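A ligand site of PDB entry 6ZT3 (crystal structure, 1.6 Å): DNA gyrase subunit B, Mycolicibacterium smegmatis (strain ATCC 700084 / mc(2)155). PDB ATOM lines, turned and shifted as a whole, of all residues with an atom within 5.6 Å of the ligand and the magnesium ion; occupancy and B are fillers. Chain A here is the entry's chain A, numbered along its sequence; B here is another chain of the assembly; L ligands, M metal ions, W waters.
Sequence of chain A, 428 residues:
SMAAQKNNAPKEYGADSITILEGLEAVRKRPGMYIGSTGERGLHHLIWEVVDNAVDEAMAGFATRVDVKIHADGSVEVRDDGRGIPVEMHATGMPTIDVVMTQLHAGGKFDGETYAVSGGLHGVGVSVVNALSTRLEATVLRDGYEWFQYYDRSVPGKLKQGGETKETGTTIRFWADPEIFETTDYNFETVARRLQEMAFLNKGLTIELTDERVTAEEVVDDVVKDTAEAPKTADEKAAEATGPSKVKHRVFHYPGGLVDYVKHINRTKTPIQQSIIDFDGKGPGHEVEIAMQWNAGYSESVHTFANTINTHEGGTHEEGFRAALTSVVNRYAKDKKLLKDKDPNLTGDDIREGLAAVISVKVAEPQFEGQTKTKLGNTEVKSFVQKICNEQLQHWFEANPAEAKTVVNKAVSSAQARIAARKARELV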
ATOM      1  N   GLU A  49     -35.077   0.369  -2.342  1.00  0.00           N
ATOM      2  CA  GLU A  49     -33.690   0.861  -2.518  1.00  0.00           C
ATOM      3  C   GLU A  49     -33.453   2.020  -1.557  1.00  0.00           C
ATOM      4  O   GLU A  49     -32.392   2.075  -0.888  1.00  0.00           O
ATOM      5  CB  GLU A  49     -33.379   1.259  -3.956  1.00  0.00           C
ATOM      6  CG  GLU A  49     -33.291   0.084  -4.921  1.00  0.00           C
ATOM      7  CD  GLU A  49     -32.116  -0.874  -4.730  1.00  0.00           C
ATOM      8  OE1 GLU A  49     -31.337  -0.701  -3.749  1.00  0.00           O
ATOM      9  OE2 GLU A  49     -31.980  -1.788  -5.565  1.00  0.00           O
ATOM     10  N   VAL A  50     -34.417   2.938  -1.469  1.00  0.00           N
ATOM     11  CA  VAL A  50     -34.236   4.153  -0.639  1.00  0.00           C
ATOM     12  C   VAL A  50     -34.286   3.761   0.841  1.00  0.00           C
ATOM     13  O   VAL A  50     -33.431   4.245   1.604  1.00  0.00           O
ATOM     14  CB  VAL A  50     -35.279   5.218  -1.000  1.00  0.00           C
ATOM     15  CG1 VAL A  50     -35.085   6.434  -0.109  1.00  0.00           C
ATOM     16  CG2 VAL A  50     -35.179   5.589  -2.475  1.00  0.00           C
ATOM     17  N   ASP A  52     -33.643   0.788   2.175  1.00  0.00           N
ATOM     18  CA  ASP A  52     -32.444  -0.049   2.475  1.00  0.00           C
ATOM     19  C   ASP A  52     -31.274   0.863   2.861  1.00  0.00           C
ATOM     20  O   ASP A  52     -30.535   0.510   3.788  1.00  0.00           O
ATOM     21  CB  ASP A  52     -32.024  -0.937   1.307  1.00  0.00           C
ATOM     22  CG  ASP A  52     -32.916  -2.130   0.993  1.00  0.00           C
ATOM     23  OD1 ASP A  52     -33.804  -2.473   1.827  1.00  0.00           O
ATOM     24  OD2 ASP A  52     -32.711  -2.732  -0.091  1.00  0.00           O
ATOM     25  N   ASN A  53     -31.106   2.003   2.180  1.00  0.00           N
ATOM     26  CA  ASN A  53     -29.971   2.925   2.476  1.00  0.00           C
ATOM     27  C   ASN A  53     -30.144   3.527   3.867  1.00  0.00           C
ATOM     28  O   ASN A  53     -29.144   3.716   4.576  1.00  0.00           O
ATOM     29  CB  ASN A  53     -29.848   3.996   1.411  1.00  0.00           C
ATOM     30  CG  ASN A  53     -29.388   3.456   0.085  1.00  0.00           C
ATOM     31  OD1 ASN A  53     -28.773   2.371   0.042  1.00  0.00           O
ATOM     32  ND2 ASN A  53     -29.671   4.188  -0.983  1.00  0.00           N
ATOM     33  N   ALA A  54     -31.374   3.833   4.260  1.00  0.00           N
ATOM     34  CA  ALA A  54     -31.664   4.345   5.611  1.00  0.00           C
ATOM     35  C   ALA A  54     -31.411   3.242   6.649  1.00  0.00           C
ATOM     36  O   ALA A  54     -30.742   3.525   7.675  1.00  0.00           O
ATOM     37  CB  ALA A  54     -33.081   4.851   5.659  1.00  0.00           C
ATOM     38  N   ASP A  56     -29.334   0.804   6.331  1.00  0.00           N
ATOM     39  CA  ASP A  56     -27.858   0.620   6.406  1.00  0.00           C
ATOM     40  C   ASP A  56     -27.262   1.625   7.395  1.00  0.00           C
ATOM     41  O   ASP A  56     -26.399   1.229   8.180  1.00  0.00           O
ATOM     42  CB  ASP A  56     -27.233   0.694   5.010  1.00  0.00           C
ATOM     43  CG  ASP A  56     -27.505  -0.526   4.158  1.00  0.00           C
ATOM     44  OD1 ASP A  56     -27.957  -1.562   4.718  1.00  0.00           O
ATOM     45  OD2 ASP A  56     -27.227  -0.462   2.923  1.00  0.00           O
ATOM     46  N   GLU A  57     -27.769   2.873   7.443  1.00  0.00           N
ATOM     47  CA  GLU A  57     -27.321   3.860   8.460  1.00  0.00           C
ATOM     48  C   GLU A  57     -27.678   3.358   9.864  1.00  0.00           C
ATOM     49  O   GLU A  57     -26.908   3.592  10.797  1.00  0.00           O
ATOM     50  CB  GLU A  57     -27.901   5.263   8.183  1.00  0.00           C
ATOM     51  CG  GLU A  57     -27.180   5.996   7.066  1.00  0.00           C
ATOM     52  CD  GLU A  57     -25.753   6.441   7.370  1.00  0.00           C
ATOM     53  OE1 GLU A  57     -25.497   6.970   8.500  1.00  0.00           O
ATOM     54  OE2 GLU A  57     -24.885   6.279   6.496  1.00  0.00           O
ATOM     55  N   ASP A  80     -34.190   9.657   7.256  1.00  0.00           N
ATOM     56  CA  ASP A  80     -33.435   9.000   8.351  1.00  0.00           C
ATOM     57  C   ASP A  80     -32.662  10.065   9.129  1.00  0.00           C
ATOM     58  O   ASP A  80     -32.389  11.158   8.581  1.00  0.00           O
ATOM     59  CB  ASP A  80     -32.574   7.880   7.779  1.00  0.00           C
ATOM     60  CG  ASP A  80     -31.373   8.377   6.989  1.00  0.00           C
ATOM     61  OD1 ASP A  80     -30.485   8.989   7.606  1.00  0.00           O
ATOM     62  OD2 ASP A  80     -31.356   8.154   5.762  1.00  0.00           O
ATOM     63  N   ARG A  83     -26.044   9.748   9.089  1.00  0.00           N
ATOM     64  CA  ARG A  83     -24.883  10.664   8.924  1.00  0.00           C
ATOM     65  C   ARG A  83     -25.119  11.686   7.796  1.00  0.00           C
ATOM     66  O   ARG A  83     -24.343  12.667   7.736  1.00  0.00           O
ATOM     67  CB  ARG A  83     -23.617   9.867   8.627  1.00  0.00           C
ATOM     68  CG  ARG A  83     -23.088   9.157   9.865  1.00  0.00           C
ATOM     69  CD  ARG A  83     -21.999   8.158   9.534  1.00  0.00           C
ATOM     70  NE  ARG A  83     -22.544   7.038   8.776  1.00  0.00           N
ATOM     71  CZ  ARG A  83     -21.828   6.010   8.356  1.00  0.00           C
ATOM     72  NH1 ARG A  83     -20.534   5.941   8.640  1.00  0.00           N
ATOM     73  NH2 ARG A  83     -22.400   5.045   7.652  1.00  0.00           N
ATOM     74  N   GLY A  84     -26.102  11.458   6.936  1.00  0.00           N
ATOM     75  CA  GLY A  84     -26.301  12.268   5.721  1.00  0.00           C
ATOM     76  C   GLY A  84     -25.421  11.806   4.566  1.00  0.00           C
ATOM     77  O   GLY A  84     -24.276  11.343   4.804  1.00  0.00           O
ATOM     78  N   ILE A  85     -25.924  11.929   3.333  1.00  0.00           N
ATOM     79  CA  ILE A  85     -25.100  11.732   2.114  1.00  0.00           C
ATOM     80  C   ILE A  85     -24.133  12.914   2.027  1.00  0.00           C
ATOM     81  O   ILE A  85     -24.560  14.065   2.095  1.00  0.00           O
ATOM     82  CB  ILE A  85     -25.964  11.648   0.845  1.00  0.00           C
ATOM     83  CG1 ILE A  85     -27.026  10.541   0.938  1.00  0.00           C
ATOM     84  CG2 ILE A  85     -25.064  11.491  -0.376  1.00  0.00           C
ATOM     85  CD1 ILE A  85     -28.050  10.547  -0.168  1.00  0.00           C
ATOM     86  N   PRO A  86     -22.816  12.697   1.868  1.00  0.00           N
ATOM     87  CA  PRO A  86     -21.909  13.808   1.663  1.00  0.00           C
ATOM     88  C   PRO A  86     -22.323  14.693   0.475  1.00  0.00           C
ATOM     89  O   PRO A  86     -22.722  14.168  -0.562  1.00  0.00           O
ATOM     90  CB  PRO A  86     -20.555  13.131   1.394  1.00  0.00           C
ATOM     91  CG  PRO A  86     -20.674  11.812   2.107  1.00  0.00           C
ATOM     92  CD  PRO A  86     -22.116  11.395   1.870  1.00  0.00           C
ATOM     93  N   VAL A 100     -23.496   9.706  -6.653  1.00  0.00           N
ATOM     94  CA  VAL A 100     -24.245   8.475  -6.341  1.00  0.00           C
ATOM     95  C   VAL A 100     -25.576   8.496  -7.137  1.00  0.00           C
ATOM     96  O   VAL A 100     -25.919   7.438  -7.717  1.00  0.00           O
ATOM     97  CB  VAL A 100     -24.392   8.253  -4.823  1.00  0.00           C
ATOM     98  CG1 VAL A 100     -23.024   7.994  -4.192  1.00  0.00           C
ATOM     99  CG2 VAL A 100     -25.113   9.373  -4.097  1.00  0.00           C
ATOM    100  N   ALA A 106     -21.113   3.245  -7.935  1.00  0.00           N
ATOM    101  CA  ALA A 106     -20.532   4.335  -7.132  1.00  0.00           C
ATOM    102  C   ALA A 106     -21.138   4.309  -5.726  1.00  0.00           C
ATOM    103  O   ALA A 106     -22.370   4.313  -5.604  1.00  0.00           O
ATOM    104  CB  ALA A 106     -20.760   5.655  -7.805  1.00  0.00           C
ATOM    105  N   GLY A 107     -20.309   4.226  -4.688  1.00  0.00           N
ATOM    106  CA  GLY A 107     -20.850   4.190  -3.325  1.00  0.00           C
ATOM    107  C   GLY A 107     -19.799   3.997  -2.250  1.00  0.00           C
ATOM    108  O   GLY A 107     -18.592   3.948  -2.566  1.00  0.00           O
ATOM    109  N   GLY A 108     -20.288   3.927  -1.017  1.00  0.00           N
ATOM    110  CA  GLY A 108     -19.481   3.809   0.207  1.00  0.00           C
ATOM    111  C   GLY A 108     -19.462   2.404   0.769  1.00  0.00           C
ATOM    112  O   GLY A 108     -18.972   2.262   1.885  1.00  0.00           O
ATOM    113  N   LYS A 109     -19.976   1.405   0.027  1.00  0.00           N
ATOM    114  CA  LYS A 109     -20.148   0.023   0.552  1.00  0.00           C
ATOM    115  C   LYS A 109     -19.295  -0.990  -0.212  1.00  0.00           C
ATOM    116  O   LYS A 109     -19.597  -2.180  -0.115  1.00  0.00           O
ATOM    117  CB  LYS A 109     -21.636  -0.330   0.544  1.00  0.00           C
ATOM    118  CG  LYS A 109     -22.444   0.559   1.486  1.00  0.00           C
ATOM    119  CD  LYS A 109     -23.947   0.479   1.323  1.00  0.00           C
ATOM    120  CE  LYS A 109     -24.654   1.601   2.039  1.00  0.00           C
ATOM    121  NZ  LYS A 109     -26.089   1.649   1.699  1.00  0.00           N
ATOM    122  N   THR A 114     -17.030   2.428   5.917  1.00  0.00           N
ATOM    123  CA  THR A 114     -18.152   3.396   6.087  1.00  0.00           C
ATOM    124  C   THR A 114     -19.351   2.657   6.691  1.00  0.00           C
ATOM    125  O   THR A 114     -20.028   3.257   7.549  1.00  0.00           O
ATOM    126  CB  THR A 114     -18.468   4.102   4.768  1.00  0.00           C
ATOM    127  OG1 THR A 114     -17.241   4.603   4.225  1.00  0.00           O
ATOM    128  CG2 THR A 114     -19.447   5.237   4.954  1.00  0.00           C
ATOM    129  N   TYR A 115     -19.583   1.424   6.236  1.00  0.00           N
ATOM    130  CA  TYR A 115     -20.618   0.473   6.712  1.00  0.00           C
ATOM    131  C   TYR A 115     -19.967  -0.900   6.861  1.00  0.00           C
ATOM    132  O   TYR A 115     -19.571  -1.504   5.849  1.00  0.00           O
ATOM    133  CB  TYR A 115     -21.774   0.384   5.718  1.00  0.00           C
ATOM    134  CG  TYR A 115     -22.484   1.676   5.366  1.00  0.00           C
ATOM    135  CD1 TYR A 115     -22.001   2.523   4.385  1.00  0.00           C
ATOM    136  CD2 TYR A 115     -23.689   2.009   5.970  1.00  0.00           C
ATOM    137  CE1 TYR A 115     -22.672   3.683   4.015  1.00  0.00           C
ATOM    138  CE2 TYR A 115     -24.374   3.176   5.631  1.00  0.00           C
ATOM    139  CZ  TYR A 115     -23.862   4.013   4.638  1.00  0.00           C
ATOM    140  OH  TYR A 115     -24.491   5.174   4.268  1.00  0.00           O
ATOM    141  N   GLY A 119     -26.880  -3.971   3.648  1.00  0.00           N
ATOM    142  CA  GLY A 119     -27.622  -4.583   2.530  1.00  0.00           C
ATOM    143  C   GLY A 119     -27.134  -4.030   1.208  1.00  0.00           C
ATOM    144  O   GLY A 119     -27.129  -4.782   0.214  1.00  0.00           O
ATOM    145  N   GLY A 120     -26.721  -2.771   1.209  1.00  0.00           N
ATOM    146  CA  GLY A 120     -26.110  -2.115   0.033  1.00  0.00           C
ATOM    147  C   GLY A 120     -24.736  -2.719  -0.272  1.00  0.00           C
ATOM    148  O   GLY A 120     -23.959  -2.943   0.673  1.00  0.00           O
ATOM    149  N   LEU A 121     -24.415  -2.912  -1.552  1.00  0.00           N
ATOM    150  CA  LEU A 121     -23.066  -3.384  -1.961  1.00  0.00           C
ATOM    151  C   LEU A 121     -22.732  -3.047  -3.412  1.00  0.00           C
ATOM    152  O   LEU A 121     -21.544  -3.182  -3.768  1.00  0.00           O
ATOM    153  CB  LEU A 121     -22.936  -4.885  -1.707  1.00  0.00           C
ATOM    154  CG  LEU A 121     -23.576  -5.827  -2.724  1.00  0.00           C
ATOM    155  CD1 LEU A 121     -23.172  -7.265  -2.415  1.00  0.00           C
ATOM    156  CD2 LEU A 121     -25.086  -5.706  -2.751  1.00  0.00           C
ATOM    157  N   HIS A 122     -23.706  -2.685  -4.256  1.00  0.00           N
ATOM    158  CA  HIS A 122     -23.444  -2.529  -5.716  1.00  0.00           C
ATOM    159  C   HIS A 122     -23.126  -1.102  -6.129  1.00  0.00           C
ATOM    160  O   HIS A 122     -22.591  -0.951  -7.231  1.00  0.00           O
ATOM    161  CB  HIS A 122     -24.601  -3.077  -6.534  1.00  0.00           C
ATOM    162  CG  HIS A 122     -24.803  -4.543  -6.386  1.00  0.00           C
ATOM    163  ND1 HIS A 122     -26.044  -5.108  -6.450  1.00  0.00           N
ATOM    164  CD2 HIS A 122     -23.931  -5.543  -6.153  1.00  0.00           C
ATOM    165  CE1 HIS A 122     -25.947  -6.399  -6.293  1.00  0.00           C
ATOM    166  NE2 HIS A 122     -24.651  -6.695  -6.131  1.00  0.00           N
ATOM    167  N   GLY A 123     -23.511  -0.108  -5.338  1.00  0.00           N
ATOM    168  CA  GLY A 123     -23.405   1.321  -5.730  1.00  0.00           C
ATOM    169  C   GLY A 123     -24.347   1.664  -6.875  1.00  0.00           C
ATOM    170  O   GLY A 123     -23.956   2.490  -7.737  1.00  0.00           O
ATOM    171  N   VAL A 124     -25.567   1.106  -6.866  1.00  0.00           N
ATOM    172  CA  VAL A 124     -26.531   1.216  -8.010  1.00  0.00           C
ATOM    173  C   VAL A 124     -27.896   1.747  -7.537  1.00  0.00           C
ATOM    174  O   VAL A 124     -28.495   2.527  -8.278  1.00  0.00           O
ATOM    175  CB  VAL A 124     -26.644  -0.152  -8.690  1.00  0.00           C
ATOM    176  CG1 VAL A 124     -27.876  -0.313  -9.535  1.00  0.00           C
ATOM    177  CG2 VAL A 124     -25.388  -0.474  -9.506  1.00  0.00           C
ATOM    178  N   GLY A 125     -28.360   1.355  -6.354  1.00  0.00           N
ATOM    179  CA  GLY A 125     -29.749   1.534  -5.897  1.00  0.00           C
ATOM    180  C   GLY A 125     -30.323   2.924  -6.146  1.00  0.00           C
ATOM    181  O   GLY A 125     -31.353   3.027  -6.841  1.00  0.00           O
ATOM    182  N   VAL A 126     -29.695   3.953  -5.591  1.00  0.00           N
ATOM    183  CA  VAL A 126     -30.270   5.335  -5.606  1.00  0.00           C
ATOM    184  C   VAL A 126     -30.164   5.925  -7.022  1.00  0.00           C
ATOM    185  O   VAL A 126     -31.055   6.680  -7.400  1.00  0.00           O
ATOM    186  CB  VAL A 126     -29.621   6.192  -4.495  1.00  0.00           C
ATOM    187  CG1 VAL A 126     -28.426   7.003  -4.970  1.00  0.00           C
ATOM    188  CG2 VAL A 126     -30.659   7.063  -3.804  1.00  0.00           C
ATOM    189  N   SER A 127     -29.187   5.477  -7.835  1.00  0.00           N
ATOM    190  CA  SER A 127     -29.075   5.879  -9.252  1.00  0.00           C
ATOM    191  C   SER A 127     -30.238   5.276 -10.052  1.00  0.00           C
ATOM    192  O   SER A 127     -30.740   5.958 -10.957  1.00  0.00           O
ATOM    193  CB  SER A 127     -27.750   5.533  -9.879  1.00  0.00           C
ATOM    194  OG  SER A 127     -27.093   4.495  -9.174  1.00  0.00           O
ATOM    195  N   THR A 170     -30.701  12.348   6.162  1.00  0.00           N
ATOM    196  CA  THR A 170     -31.022  12.373   4.714  1.00  0.00           C
ATOM    197  C   THR A 170     -32.523  12.219   4.555  1.00  0.00           C
ATOM    198  O   THR A 170     -33.092  11.269   5.164  1.00  0.00           O
ATOM    199  CB  THR A 170     -30.315  11.245   3.955  1.00  0.00           C
ATOM    200  OG1 THR A 170     -28.912  11.364   4.188  1.00  0.00           O
ATOM    201  CG2 THR A 170     -30.586  11.273   2.466  1.00  0.00           C
ATOM    202  N   GLN A 371     -29.450  -7.091  -8.600  1.00  0.00           N
ATOM    203  CA  GLN A 371     -29.835  -5.877  -7.853  1.00  0.00           C
ATOM    204  C   GLN A 371     -31.107  -6.132  -7.020  1.00  0.00           C
ATOM    205  O   GLN A 371     -31.243  -5.473  -5.985  1.00  0.00           O
ATOM    206  CB  GLN A 371     -29.992  -4.703  -8.803  1.00  0.00           C
ATOM    207  CG  GLN A 371     -30.224  -3.381  -8.063  1.00  0.00           C
ATOM    208  CD  GLN A 371     -29.013  -2.983  -7.247  1.00  0.00           C
ATOM    209  OE1 GLN A 371     -27.873  -3.360  -7.563  1.00  0.00           O
ATOM    210  NE2 GLN A 371     -29.245  -2.208  -6.196  1.00  0.00           N
ATOM    211  N   LYS A 373     -31.620  -8.854  -5.427  1.00  0.00           N
ATOM    212  CA  LYS A 373     -31.028  -9.542  -4.247  1.00  0.00           C
ATOM    213  C   LYS A 373     -31.966 -10.645  -3.753  1.00  0.00           C
ATOM    214  O   LYS A 373     -32.171 -10.762  -2.530  1.00  0.00           O
ATOM    215  CB  LYS A 373     -30.724  -8.501  -3.168  1.00  0.00           C
ATOM    216  CG  LYS A 373     -29.779  -7.401  -3.611  1.00  0.00           C
ATOM    217  CD  LYS A 373     -29.483  -6.326  -2.586  1.00  0.00           C
ATOM    218  CE  LYS A 373     -28.701  -5.177  -3.182  1.00  0.00           C
ATOM    219  NZ  LYS A 373     -28.432  -4.122  -2.203  1.00  0.00           N
ATOM    220  N   TYR B  13     -16.994   9.951   7.386  1.00  0.00           N
ATOM    221  CA  TYR B  13     -17.779   9.609   6.183  1.00  0.00           C
ATOM    222  C   TYR B  13     -17.869  10.867   5.323  1.00  0.00           C
ATOM    223  O   TYR B  13     -18.686  11.758   5.661  1.00  0.00           O
ATOM    224  CB  TYR B  13     -19.145   9.074   6.596  1.00  0.00           C
ATOM    225  CG  TYR B  13     -20.116   8.764   5.482  1.00  0.00           C
ATOM    226  CD1 TYR B  13     -19.719   8.619   4.161  1.00  0.00           C
ATOM    227  CD2 TYR B  13     -21.442   8.540   5.769  1.00  0.00           C
ATOM    228  CE1 TYR B  13     -20.634   8.312   3.171  1.00  0.00           C
ATOM    229  CE2 TYR B  13     -22.364   8.222   4.797  1.00  0.00           C
ATOM    230  CZ  TYR B  13     -21.961   8.112   3.483  1.00  0.00           C
ATOM    231  OH  TYR B  13     -22.877   7.817   2.506  1.00  0.00           O
ATOM    232  N   ILE B  18     -16.712   7.565  -1.001  1.00  0.00           N
ATOM    233  CA  ILE B  18     -17.480   7.139  -2.212  1.00  0.00           C
ATOM    234  C   ILE B  18     -16.477   6.816  -3.325  1.00  0.00           C
ATOM    235  O   ILE B  18     -15.760   7.726  -3.760  1.00  0.00           O
ATOM    236  CB  ILE B  18     -18.487   8.204  -2.665  1.00  0.00           C
ATOM    237  CG1 ILE B  18     -19.499   8.583  -1.580  1.00  0.00           C
ATOM    238  CG2 ILE B  18     -19.162   7.759  -3.941  1.00  0.00           C
ATOM    239  CD1 ILE B  18     -20.133   7.437  -0.880  1.00  0.00           C
HETATM  240  P1  LIG L   1     -26.753  -0.943  -3.621  1.00  0.00           P
HETATM  241  O1  LIG L   1     -26.779  -0.638  -5.080  1.00  0.00           O
HETATM  242  O2  LIG L   1     -26.581  -2.421  -3.331  1.00  0.00           O
HETATM  243  O3  LIG L   1     -27.902  -0.385  -2.876  1.00  0.00           O
HETATM  244  P2  LIG L   1     -25.255   1.192  -2.260  1.00  0.00           P
HETATM  245  O4  LIG L   1     -23.834   1.566  -1.930  1.00  0.00           O
HETATM  246  O5  LIG L   1     -26.220   1.406  -1.139  1.00  0.00           O
HETATM  247  N1  LIG L   1     -25.409  -0.243  -2.974  1.00  0.00           N
HETATM  248  P3  LIG L   1     -26.784   3.300  -3.519  1.00  0.00           P
HETATM  249  O6  LIG L   1     -26.824   3.816  -4.921  1.00  0.00           O
HETATM  250  O7  LIG L   1     -28.098   2.860  -2.941  1.00  0.00           O
HETATM  251  O8  LIG L   1     -25.713   2.104  -3.514  1.00  0.00           O
HETATM  252  O9  LIG L   1     -26.069   4.346  -2.530  1.00  0.00           O
HETATM  253  C1  LIG L   1     -24.840   4.967  -2.925  1.00  0.00           C
HETATM  254  C2  LIG L   1     -24.146   5.490  -1.703  1.00  0.00           C
HETATM  255  O10 LIG L   1     -24.818   6.694  -1.255  1.00  0.00           O
HETATM  256  C3  LIG L   1     -24.149   4.590  -0.477  1.00  0.00           C
HETATM  257  O11 LIG L   1     -23.146   3.570  -0.526  1.00  0.00           O
HETATM  258  C4  LIG L   1     -23.844   5.615   0.608  1.00  0.00           C
HETATM  259  O12 LIG L   1     -22.460   5.908   0.644  1.00  0.00           O
HETATM  260  C5  LIG L   1     -24.685   6.803   0.151  1.00  0.00           C
HETATM  261  N2  LIG L   1     -26.058   6.885   0.720  1.00  0.00           N
HETATM  262  C6  LIG L   1     -27.244   6.546   0.101  1.00  0.00           C
HETATM  263  N3  LIG L   1     -28.290   6.731   0.878  1.00  0.00           N
HETATM  264  C7  LIG L   1     -27.757   7.221   2.061  1.00  0.00           C
HETATM  265  C8  LIG L   1     -28.360   7.615   3.273  1.00  0.00           C
HETATM  266  N4  LIG L   1     -29.668   7.542   3.501  1.00  0.00           N
HETATM  267  N5  LIG L   1     -27.541   8.072   4.255  1.00  0.00           N
HETATM  268  C9  LIG L   1     -26.225   8.126   4.013  1.00  0.00           C
HETATM  269  N6  LIG L   1     -25.539   7.766   2.921  1.00  0.00           N
HETATM  270  C10 LIG L   1     -26.386   7.316   1.971  1.00  0.00           C
HETATM  271 MG    MG M   1     -28.338   1.171  -1.552  1.00  0.00          MG
HETATM  272  O   HOH W   1     -21.236   1.037  -2.615  1.00  0.00           O
HETATM  273  O   HOH W   2     -26.852   4.142   2.993  1.00  0.00           O
HETATM  274  O   HOH W   3     -28.261   9.694   6.320  1.00  0.00           O
HETATM  275  O   HOH W   4     -30.284  -2.200  -1.282  1.00  0.00           O
HETATM  276  O   HOH W   5     -32.228   6.775   2.080  1.00  0.00           O
HETATM  277  O   HOH W   6     -30.321   1.131  -2.106  1.00  0.00           O
HETATM  278  O   HOH W   7     -28.649  -0.360  -0.005  1.00  0.00           O
HETATM  279  O   HOH W   8     -30.822   6.822  -0.427  1.00  0.00           O
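Glu 49 touches the ligand.
Glu 57 touches the ligand.
Gly 84 touches the ligand (C to C9, 3.8 Å).
CG1 of Ile 85 touches C10 of the ligand (3.4 Å).
CG1 of Val 100 touches O10 of the ligand, 3.7 Å away.
Ala 106 touches the ligand (O to C1, 3.7 Å).
CA of Gly 107 touches O11 of the ligand (3.7 Å).
Gly 120 touches the ligand (CA to O2, 3.4 Å).
OG1 of Thr 170 touches N5 of the ligand (3.6 Å).
CD1 of Ile 18 of chain B touches O12 of the ligand, at 3.2 Å.
Hydrophobic or aromatic side chains that line the ligand: Ile 85, Val 100, Leu 121, His 122, Val 124, Val 126, Tyr 13 of chain B and Ile 18 of chain B.
Of the 33 residues printed, 24 come within 4 Å of the ligand.
The nearest printed residue that does not touch the ligand is Ser 127 (4.1 Å).
The magnesium ion is bound by OD1 of Asn 53 (2.0 Å), water W6 (2.1 Å), O3 of the ligand (2.1 Å), O5 of the ligand (2.2 Å), water W7 (2.2 Å) and O7 of the ligand (2.2 Å).
The side-chain hydroxyl (OH) of Tyr 115 lies within hydrogen-bond range of a nitrogen (N6) of the ligand.
A nitrogen (N4) of the ligand sits at hydrogen-bond distance from the side-chain carboxylate (OD2) of Asp 80 (2.9 Å).
An oxygen (O1) of the ligand sits at hydrogen-bond distance from the backbone NH (N) of Gly 123.
The backbone NH (N) of Gly 125 sits at hydrogen-bond distance from an oxygen (O1) of the ligand.
O1 of the ligand lies within hydrogen-bond range of NE2 of Gln 371 (3.1 Å).
The backbone NH (N) of Val 126 lies within hydrogen-bond range of an oxygen (O6) of the ligand, 3.0 Å away.
O11 of the ligand lies within hydrogen-bond range of N of Gly 108, at 2.9 Å.
N of Leu 121 sits at hydrogen-bond distance from O2 of the ligand (2.8 Å).
An oxygen (O1) of the ligand sits at hydrogen-bond distance from the backbone NH (N) of Val 124.
NZ of Lys 373 lies within salt-bridge range of O2 of the ligand (2.8 Å).
An oxygen (O5) of the ligand sits close to the side-chain amino group (NZ) of Lys 109 (2.9 Å).
OH of Tyr 13 of chain B is in hydrogen-bond range of N6 of the ligand, 2.7 Å away.
The backbone NH (N) of His 122 sits at hydrogen-bond distance from an oxygen (O2) of the ligand (3.0 Å).
Water W3 lies within hydrogen-bond range of OD1 of Asp 80 (2.7 Å), N5 of the ligand (2.7 Å), OG1 of Thr 170 (2.8 Å) and N of Gly 84 (2.9 Å).
Water W1 lies within hydrogen-bond range of an oxygen (O4) of the ligand (2.7 Å), the backbone NH of Lys 109 (3.0 Å) and the backbone NH of Gly 108 (3.4 Å).
Water W8 lies within hydrogen-bond range of a nitrogen (N3) of the ligand (2.8 Å) and the side-chain amide nitrogen of Asn 53 (2.9 Å).
Water W5 bridges the backbone carbonyl oxygen (O) of Val 50 and a nitrogen (N4) of the ligand.
Water W2 lies within hydrogen-bond range of the backbone carbonyl oxygen (O) of Asn 53, the side-chain hydroxyl (OH) of Tyr 115 and the side-chain amino group (NZ) of Lys 109.
Water W4 lies within hydrogen-bond range of OD2 of Asp 52 (2.8 Å), NZ of Lys 373 (2.8 Å) and OE1 of Glu 49 (3.1 Å).
Lys 109 touches the magnesium ion (NZ to MG, 3.98 Å).
Of the 33 residues printed, 2 come within 4 Å of the magnesium ion.
The nearest printed residue that does not touch the magnesium ion is Glu 49 (4.2 Å).
The backbone carbonyl oxygen (O) of Thr 170 sits at hydrogen-bond distance from the backbone NH (N) of Asp 80, 2.9 Å away.
The side-chain hydroxyl of Thr 170 is in hydrogen-bond range of the backbone NH of Ile 85, at 3.2 Å.
NZ of Lys 373 is in hydrogen-bond range of O of Gly 119 (2.8 Å).
OE2 of Glu 49 sits at hydrogen-bond distance from NE2 of Gln 371, 2.8 Å away.
The side-chain amide oxygen (OE1) of Gln 371 sits at hydrogen-bond distance from a ring nitrogen (ND1) of His 122 (2.8 Å).
The backbone carbonyl oxygen of Val 124 sits at hydrogen-bond distance from the side-chain hydroxyl of Ser 127, 2.6 Å away.
OE1 of Glu 57 lies within salt-bridge range of NE of Arg 83.
The backbone NH of Gly 120 is in hydrogen-bond range of the side-chain carboxylate of Asp 56, 2.9 Å away.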
